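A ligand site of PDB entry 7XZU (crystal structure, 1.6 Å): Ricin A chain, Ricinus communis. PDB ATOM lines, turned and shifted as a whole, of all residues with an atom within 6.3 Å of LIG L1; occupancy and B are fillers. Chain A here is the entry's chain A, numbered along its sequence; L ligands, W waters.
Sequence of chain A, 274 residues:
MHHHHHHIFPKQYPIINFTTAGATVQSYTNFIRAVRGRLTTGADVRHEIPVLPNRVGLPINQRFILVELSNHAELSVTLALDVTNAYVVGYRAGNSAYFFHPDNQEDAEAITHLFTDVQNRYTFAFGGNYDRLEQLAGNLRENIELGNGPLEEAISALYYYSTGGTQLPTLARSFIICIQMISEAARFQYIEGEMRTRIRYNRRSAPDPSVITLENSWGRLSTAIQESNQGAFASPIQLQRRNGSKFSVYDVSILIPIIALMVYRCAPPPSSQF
Water W4 lies within hydrogen-bond range of an oxygen (O1) of LIG L1 (2.9 Å), the backbone NH (N) of Asp 131 (3.0 Å) and the backbone NH (N) of Tyr 130 (3.4 Å).
Water W1 lies within hydrogen-bond range of O3 of LG2 L2 and OD1 of Asn 129.
Water W2 lies within hydrogen-bond range of OE2 of Glu 184 and O of Glu 215.
The backbone carbonyl oxygen of Ala 86 lies close to an oxygen (O2) of LIG L1 (3.5 Å).
Merely in contact with LIG L1: Tyr 87 (3.3 Å), Phe 100 (3.6 Å), Asn 129 (3.6 Å), Ile 179 (3.4 Å), Ser 183 (3.5 Å) and Glu 184 (3.7 Å).
Hydrophobic or aromatic side chains that line LIG L1: Tyr 87, Val 88, Phe 100, Tyr 130 and Ile 179.
Of the 19 residues printed, 11 come within 4 Å of LIG L1.
OH of Tyr 87 lies close to N of Gly 128 (3.4 Å).
NH1 of Arg 187 is in salt-bridge range of OE1 of Glu 184 (3.1 Å).
The guanidinium group of Arg 187 is in hydrogen-bond range of the backbone carbonyl oxygen of Asn 85 (2.8 Å).
The side-chain hydroxyl of Tyr 130 sits at hydrogen-bond distance from the side-chain carboxylate of Glu 184, at 2.6 Å.
The side-chain hydroxyl (OH) of Tyr 87 is in hydrogen-bond range of the side-chain amide oxygen (OD1) of Asn 129, at 2.8 Å.
N of Tyr 87 is in hydrogen-bond range of OD1 of Asn 85 (3.0 Å).
OG of Ser 183 is in hydrogen-bond range of O of Ala 86.
N of Phe 100 is in hydrogen-bond range of O of Val 89, 3.0 Å away.
The backbone carbonyl oxygen (O) of Gly 128 is in hydrogen-bond range of a nitrogen (N4) of LIG L1 (3.1 Å).
The guanidinium group of Arg 187 lies within hydrogen-bond range of an oxygen (O2) of LIG L1 (2.8 Å).
An oxygen (O1) of LIG L1 sits at hydrogen-bond distance from the backbone NH (N) of Tyr 130, 2.9 Å away.
O of Val 88 sits at hydrogen-bond distance from N4 of LIG L1, 2.9 Å away.
A nitrogen (N2) of LG2 L2 is in hydrogen-bond range of the side-chain amide nitrogen (ND2) of Asn 85 (3.1 Å).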
ATOM      1  N   ASN A  85     -15.696  33.505 -10.602  1.00  0.00           N
ATOM      2  CA  ASN A  85     -15.755  32.096 -11.035  1.00  0.00           C
ATOM      3  C   ASN A  85     -14.638  31.212 -10.485  1.00  0.00           C
ATOM      4  O   ASN A  85     -14.591  30.024 -10.803  1.00  0.00           O
ATOM      5  CB  ASN A  85     -15.814  31.998 -12.563  1.00  0.00           C
ATOM      6  CG  ASN A  85     -14.651  32.699 -13.236  1.00  0.00           C
ATOM      7  OD1 ASN A  85     -13.674  33.089 -12.590  1.00  0.00           O
ATOM      8  ND2 ASN A  85     -14.758  32.890 -14.542  1.00  0.00           N
ATOM      9  N   ALA A  86     -13.770  31.804  -9.662  1.00  0.00           N
ATOM     10  CA  ALA A  86     -12.552  31.147  -9.116  1.00  0.00           C
ATOM     11  C   ALA A  86     -11.524  30.731 -10.196  1.00  0.00           C
ATOM     12  O   ALA A  86     -10.606  29.962  -9.924  1.00  0.00           O
ATOM     13  CB  ALA A  86     -12.907  29.988  -8.184  1.00  0.00           C
ATOM     14  N   TYR A  87     -11.670  31.271 -11.406  1.00  0.00           N
ATOM     15  CA  TYR A  87     -10.810  30.929 -12.543  1.00  0.00           C
ATOM     16  C   TYR A  87      -9.388  31.441 -12.329  1.00  0.00           C
ATOM     17  O   TYR A  87      -9.195  32.601 -11.951  1.00  0.00           O
ATOM     18  CB  TYR A  87     -11.404  31.523 -13.822  1.00  0.00           C
ATOM     19  CG  TYR A  87     -10.875  30.961 -15.118  1.00  0.00           C
ATOM     20  CD1 TYR A  87      -9.737  31.510 -15.730  1.00  0.00           C
ATOM     21  CD2 TYR A  87     -11.533  29.899 -15.753  1.00  0.00           C
ATOM     22  CE1 TYR A  87      -9.257  30.992 -16.920  1.00  0.00           C
ATOM     23  CE2 TYR A  87     -11.068  29.392 -16.956  1.00  0.00           C
ATOM     24  CZ  TYR A  87      -9.926  29.944 -17.531  1.00  0.00           C
ATOM     25  OH  TYR A  87      -9.449  29.443 -18.709  1.00  0.00           O
ATOM     26  N   VAL A  88      -8.409  30.556 -12.532  1.00  0.00           N
ATOM     27  CA  VAL A  88      -6.994  30.928 -12.453  1.00  0.00           C
ATOM     28  C   VAL A  88      -6.646  31.621 -13.773  1.00  0.00           C
ATOM     29  O   VAL A  88      -6.577  30.988 -14.820  1.00  0.00           O
ATOM     30  CB  VAL A  88      -6.080  29.701 -12.220  1.00  0.00           C
ATOM     31  CG1 VAL A  88      -4.617  30.117 -12.143  1.00  0.00           C
ATOM     32  CG2 VAL A  88      -6.484  28.967 -10.944  1.00  0.00           C
ATOM     33  N   VAL A  89      -6.447  32.942 -13.714  1.00  0.00           N
ATOM     34  CA  VAL A  89      -6.231  33.756 -14.913  1.00  0.00           C
ATOM     35  C   VAL A  89      -4.750  33.873 -15.312  1.00  0.00           C
ATOM     36  O   VAL A  89      -4.432  34.212 -16.449  1.00  0.00           O
ATOM     37  CB  VAL A  89      -6.870  35.174 -14.825  1.00  0.00           C
ATOM     38  CG1 VAL A  89      -8.376  35.084 -14.598  1.00  0.00           C
ATOM     39  CG2 VAL A  89      -6.215  36.021 -13.745  1.00  0.00           C
ATOM     40  N   PHE A 100      -3.166  33.537 -19.138  1.00  0.00           N
ATOM     41  CA  PHE A 100      -3.850  32.802 -20.187  1.00  0.00           C
ATOM     42  C   PHE A 100      -4.505  33.765 -21.165  1.00  0.00           C
ATOM     43  O   PHE A 100      -4.862  34.882 -20.786  1.00  0.00           O
ATOM     44  CB  PHE A 100      -4.905  31.868 -19.611  1.00  0.00           C
ATOM     45  CG  PHE A 100      -4.348  30.776 -18.753  1.00  0.00           C
ATOM     46  CD1 PHE A 100      -3.481  29.816 -19.284  1.00  0.00           C
ATOM     47  CD2 PHE A 100      -4.690  30.700 -17.406  1.00  0.00           C
ATOM     48  CE1 PHE A 100      -2.956  28.806 -18.475  1.00  0.00           C
ATOM     49  CE2 PHE A 100      -4.162  29.699 -16.592  1.00  0.00           C
ATOM     50  CZ  PHE A 100      -3.298  28.743 -17.131  1.00  0.00           C
ATOM     51  N   GLY A 128      -6.908  29.045 -20.974  1.00  0.00           N
ATOM     52  CA  GLY A 128      -6.633  28.246 -19.775  1.00  0.00           C
ATOM     53  C   GLY A 128      -7.614  27.155 -19.396  1.00  0.00           C
ATOM     54  O   GLY A 128      -7.481  26.580 -18.315  1.00  0.00           O
ATOM     55  N   ASN A 129      -8.591  26.848 -20.248  1.00  0.00           N
ATOM     56  CA  ASN A 129      -9.536  25.761 -19.966  1.00  0.00           C
ATOM     57  C   ASN A 129      -8.853  24.390 -20.015  1.00  0.00           C
ATOM     58  O   ASN A 129      -7.812  24.226 -20.659  1.00  0.00           O
ATOM     59  CB  ASN A 129     -10.723  25.786 -20.943  1.00  0.00           C
ATOM     60  CG  ASN A 129     -11.638  26.984 -20.752  1.00  0.00           C
ATOM     61  OD1 ASN A 129     -11.410  27.850 -19.894  1.00  0.00           O
ATOM     62  ND2 ASN A 129     -12.689  27.046 -21.568  1.00  0.00           N
ATOM     63  N   TYR A 130      -9.447  23.417 -19.314  1.00  0.00           N
ATOM     64  CA  TYR A 130      -8.904  22.048 -19.252  1.00  0.00           C
ATOM     65  C   TYR A 130      -8.608  21.463 -20.630  1.00  0.00           C
ATOM     66  O   TYR A 130      -7.528  20.913 -20.842  1.00  0.00           O
ATOM     67  CB  TYR A 130      -9.815  21.095 -18.480  1.00  0.00           C
ATOM     68  CG  TYR A 130      -9.904  21.352 -16.985  1.00  0.00           C
ATOM     69  CD1 TYR A 130      -8.770  21.669 -16.230  1.00  0.00           C
ATOM     70  CD2 TYR A 130     -11.128  21.218 -16.329  1.00  0.00           C
ATOM     71  CE1 TYR A 130      -8.861  21.885 -14.859  1.00  0.00           C
ATOM     72  CE2 TYR A 130     -11.229  21.436 -14.954  1.00  0.00           C
ATOM     73  CZ  TYR A 130     -10.096  21.772 -14.235  1.00  0.00           C
ATOM     74  OH  TYR A 130     -10.199  21.981 -12.889  1.00  0.00           O
ATOM     75  N   ASP A 131      -9.559  21.588 -21.564  1.00  0.00           N
ATOM     76  CA  ASP A 131      -9.411  20.999 -22.906  1.00  0.00           C
ATOM     77  C   ASP A 131      -8.116  21.436 -23.606  1.00  0.00           C
ATOM     78  O   ASP A 131      -7.369  20.598 -24.117  1.00  0.00           O
ATOM     79  CB  ASP A 131     -10.660  21.169 -23.784  1.00  0.00           C
ATOM     80  CG  ASP A 131     -11.104  22.629 -23.971  1.00  0.00           C
ATOM     81  OD1 ASP A 131     -10.449  23.573 -23.469  1.00  0.00           O
ATOM     82  OD2 ASP A 131     -12.127  22.823 -24.653  1.00  0.00           O
ATOM     83  N   LEU A 133      -5.461  22.862 -22.014  1.00  0.00           N
ATOM     84  CA  LEU A 133      -4.333  22.486 -21.162  1.00  0.00           C
ATOM     85  C   LEU A 133      -3.985  21.002 -21.277  1.00  0.00           C
ATOM     86  O   LEU A 133      -2.810  20.640 -21.256  1.00  0.00           O
ATOM     87  CB  LEU A 133      -4.571  22.890 -19.697  1.00  0.00           C
ATOM     88  CG  LEU A 133      -4.585  24.384 -19.359  1.00  0.00           C
ATOM     89  CD1 LEU A 133      -4.860  24.552 -17.868  1.00  0.00           C
ATOM     90  CD2 LEU A 133      -3.291  25.104 -19.720  1.00  0.00           C
ATOM     91  N   ARG A 141      -6.936  14.945 -17.606  1.00  0.00           N
ATOM     92  CA  ARG A 141      -7.039  15.011 -16.141  1.00  0.00           C
ATOM     93  C   ARG A 141      -7.076  13.630 -15.481  1.00  0.00           C
ATOM     94  O   ARG A 141      -6.413  13.427 -14.460  1.00  0.00           O
ATOM     95  CB  ARG A 141      -8.283  15.812 -15.740  1.00  0.00           C
ATOM     96  CG  ARG A 141      -8.124  17.313 -15.801  1.00  0.00           C
ATOM     97  CD  ARG A 141      -9.478  17.971 -15.624  1.00  0.00           C
ATOM     98  NE  ARG A 141     -10.291  17.884 -16.849  1.00  0.00           N
ATOM     99  CZ  ARG A 141     -11.618  17.955 -16.890  1.00  0.00           C
ATOM    100  NH1 ARG A 141     -12.337  18.086 -15.774  1.00  0.00           N
ATOM    101  NH2 ARG A 141     -12.246  17.888 -18.068  1.00  0.00           N
ATOM    102  N   ILE A 179      -5.072  24.136 -10.559  1.00  0.00           N
ATOM    103  CA  ILE A 179      -6.477  24.491 -10.763  1.00  0.00           C
ATOM    104  C   ILE A 179      -7.383  23.569  -9.961  1.00  0.00           C
ATOM    105  O   ILE A 179      -8.296  24.017  -9.268  1.00  0.00           O
ATOM    106  CB  ILE A 179      -6.855  24.514 -12.254  1.00  0.00           C
ATOM    107  CG1 ILE A 179      -6.120  25.650 -12.975  1.00  0.00           C
ATOM    108  CG2 ILE A 179      -8.361  24.670 -12.437  1.00  0.00           C
ATOM    109  CD1 ILE A 179      -5.979  25.431 -14.463  1.00  0.00           C
ATOM    110  N   SER A 183      -8.833  25.836  -7.108  1.00  0.00           N
ATOM    111  CA  SER A 183     -10.137  26.304  -7.572  1.00  0.00           C
ATOM    112  C   SER A 183     -11.252  25.261  -7.449  1.00  0.00           C
ATOM    113  O   SER A 183     -12.333  25.577  -6.941  1.00  0.00           O
ATOM    114  CB  SER A 183     -10.044  26.851  -8.994  1.00  0.00           C
ATOM    115  OG  SER A 183      -9.101  27.910  -9.035  1.00  0.00           O
ATOM    116  N   GLU A 184     -11.004  24.029  -7.900  1.00  0.00           N
ATOM    117  CA  GLU A 184     -12.042  22.999  -7.808  1.00  0.00           C
ATOM    118  C   GLU A 184     -12.336  22.612  -6.364  1.00  0.00           C
ATOM    119  O   GLU A 184     -13.491  22.339  -6.028  1.00  0.00           O
ATOM    120  CB  GLU A 184     -11.722  21.746  -8.629  1.00  0.00           C
ATOM    121  CG  GLU A 184     -11.501  21.999 -10.107  1.00  0.00           C
ATOM    122  CD  GLU A 184     -12.749  22.401 -10.889  1.00  0.00           C
ATOM    123  OE1 GLU A 184     -13.824  22.660 -10.296  1.00  0.00           O
ATOM    124  OE2 GLU A 184     -12.637  22.490 -12.138  1.00  0.00           O
ATOM    125  N   ARG A 187     -14.537  25.289  -5.037  1.00  0.00           N
ATOM    126  CA  ARG A 187     -15.896  25.117  -5.588  1.00  0.00           C
ATOM    127  C   ARG A 187     -16.673  23.962  -4.963  1.00  0.00           C
ATOM    128  O   ARG A 187     -17.893  24.057  -4.779  1.00  0.00           O
ATOM    129  CB  ARG A 187     -15.837  24.922  -7.094  1.00  0.00           C
ATOM    130  CG  ARG A 187     -15.333  26.138  -7.869  1.00  0.00           C
ATOM    131  CD  ARG A 187     -15.156  25.765  -9.332  1.00  0.00           C
ATOM    132  NE  ARG A 187     -14.543  26.859 -10.074  1.00  0.00           N
ATOM    133  CZ  ARG A 187     -13.523  26.744 -10.914  1.00  0.00           C
ATOM    134  NH1 ARG A 187     -12.998  25.548 -11.180  1.00  0.00           N
ATOM    135  NH2 ARG A 187     -13.056  27.821 -11.530  1.00  0.00           N
ATOM    136  N   GLU A 215     -16.286  18.476 -11.838  1.00  0.00           N
ATOM    137  CA  GLU A 215     -15.572  19.598 -12.474  1.00  0.00           C
ATOM    138  C   GLU A 215     -16.263  19.989 -13.774  1.00  0.00           C
ATOM    139  O   GLU A 215     -16.525  21.175 -13.999  1.00  0.00           O
ATOM    140  CB  GLU A 215     -14.118  19.241 -12.755  1.00  0.00           C
ATOM    141  CG  GLU A 215     -13.293  18.961 -11.506  1.00  0.00           C
ATOM    142  CD  GLU A 215     -11.912  18.429 -11.809  1.00  0.00           C
ATOM    143  OE1 GLU A 215     -11.604  18.157 -12.983  1.00  0.00           O
ATOM    144  OE2 GLU A 215     -11.118  18.287 -10.856  1.00  0.00           O
ATOM    145  N   ASN A 216     -16.587  18.994 -14.593  1.00  0.00           N
ATOM    146  CA  ASN A 216     -17.238  19.227 -15.883  1.00  0.00           C
ATOM    147  C   ASN A 216     -18.646  19.804 -15.788  1.00  0.00           C
ATOM    148  O   ASN A 216     -19.136  20.408 -16.741  1.00  0.00           O
ATOM    149  CB  ASN A 216     -17.262  17.936 -16.708  1.00  0.00           C
ATOM    150  CG  ASN A 216     -15.883  17.499 -17.149  1.00  0.00           C
ATOM    151  OD1 ASN A 216     -14.925  18.274 -17.128  1.00  0.00           O
ATOM    152  ND2 ASN A 216     -15.772  16.243 -17.580  1.00  0.00           N
ATOM    153  N   SER A 217     -19.276  19.617 -14.632  1.00  0.00           N
ATOM    154  CA  SER A 217     -20.687  19.967 -14.456  1.00  0.00           C
ATOM    155  C   SER A 217     -20.921  21.213 -13.608  1.00  0.00           C
ATOM    156  O   SER A 217     -22.072  21.555 -13.355  1.00  0.00           O
ATOM    157  CB  SER A 217     -21.461  18.794 -13.844  1.00  0.00           C
ATOM    158  OG  SER A 217     -21.344  17.639 -14.657  1.00  0.00           O
HETATM  159  N1  LIG L   1     -13.749  23.328 -16.774  1.00  0.00           N
HETATM  160  C1  LIG L   1     -12.446  24.882 -14.933  1.00  0.00           C
HETATM  161  C2  LIG L   1     -10.044  27.334 -13.582  1.00  0.00           C
HETATM  162  C3  LIG L   1     -11.929  24.686 -16.229  1.00  0.00           C
HETATM  163  C4  LIG L   1      -8.435  27.734 -15.323  1.00  0.00           C
HETATM  164  N2  LIG L   1      -9.084  26.856 -16.117  1.00  0.00           N
HETATM  165  C5  LIG L   1     -14.574  22.442 -17.623  1.00  0.00           C
HETATM  166  C6  LIG L   1     -12.555  23.836 -17.160  1.00  0.00           C
HETATM  167  O1  LIG L   1     -12.102  23.716 -18.289  1.00  0.00           O
HETATM  168  N3  LIG L   1     -10.809  25.366 -16.581  1.00  0.00           N
HETATM  169  C7  LIG L   1     -10.192  26.210 -15.723  1.00  0.00           C
HETATM  170  N4  LIG L   1      -7.343  28.356 -15.751  1.00  0.00           N
HETATM  171  N5  LIG L   1      -8.895  27.986 -14.036  1.00  0.00           N
HETATM  172  O2  LIG L   1     -10.427  27.567 -12.445  1.00  0.00           O
HETATM  173  C8  LIG L   1     -10.697  26.427 -14.431  1.00  0.00           C
HETATM  174  N6  LIG L   1     -11.803  25.763 -14.049  1.00  0.00           N
HETATM  175  N1  LG2 L   2     -16.396  30.711 -17.667  1.00  0.00           N
HETATM  176  C1  LG2 L   2     -18.791  30.852 -18.255  1.00  0.00           C
HETATM  177  O1  LG2 L   2     -18.414  31.825 -18.955  1.00  0.00           O
HETATM  178  C2  LG2 L   2     -13.307  30.789 -19.454  1.00  0.00           C
HETATM  179  C3  LG2 L   2     -10.871  33.436 -18.755  1.00  0.00           C
HETATM  180  C4  LG2 L   2     -14.211  30.982 -18.407  1.00  0.00           C
HETATM  181  C5  LG2 L   2     -11.647  34.597 -16.778  1.00  0.00           C
HETATM  182  N2  LG2 L   2     -12.714  33.774 -16.706  1.00  0.00           N
HETATM  183  C6  LG2 L   2     -15.836  29.108 -14.881  1.00  0.00           C
HETATM  184  C7  LG2 L   2     -14.922  28.179 -14.364  1.00  0.00           C
HETATM  185  C8  LG2 L   2     -15.210  26.816 -14.443  1.00  0.00           C
HETATM  186  C9  LG2 L   2     -16.397  26.370 -15.052  1.00  0.00           C
HETATM  187  C10 LG2 L   2     -17.299  27.307 -15.569  1.00  0.00           C
HETATM  188  C11 LG2 L   2     -17.023  28.677 -15.494  1.00  0.00           C
HETATM  189  C12 LG2 L   2     -18.011  29.716 -16.064  1.00  0.00           C
HETATM  190  C13 LG2 L   2     -17.700  30.012 -17.546  1.00  0.00           C
HETATM  191  O2  LG2 L   2     -19.981  30.490 -18.135  1.00  0.00           O
HETATM  192  C14 LG2 L   2     -15.350  30.169 -18.329  1.00  0.00           C
HETATM  193  O3  LG2 L   2     -15.407  29.088 -18.925  1.00  0.00           O
HETATM  194  N3  LG2 L   2     -13.988  31.989 -17.522  1.00  0.00           N
HETATM  195  C15 LG2 L   2     -12.899  32.791 -17.614  1.00  0.00           C
HETATM  196  N4  LG2 L   2     -11.469  35.554 -15.883  1.00  0.00           N
HETATM  197  N5  LG2 L   2     -10.695  34.447 -17.801  1.00  0.00           N
HETATM  198  O4  LG2 L   2     -10.038  33.320 -19.654  1.00  0.00           O
HETATM  199  C16 LG2 L   2     -11.983  32.605 -18.660  1.00  0.00           C
HETATM  200  N6  LG2 L   2     -12.176  31.618 -19.556  1.00  0.00           N
HETATM  201  O   HOH W   1     -13.810  26.779 -17.823  1.00  0.00           O
HETATM  202  O   HOH W   2     -15.094  23.595 -13.219  1.00  0.00           O
HETATM  203  O   HOH W   3     -17.592  21.442 -18.921  1.00  0.00           O
HETATM  204  O   HOH W   4     -12.323  22.657 -20.965  1.00  0.00           O
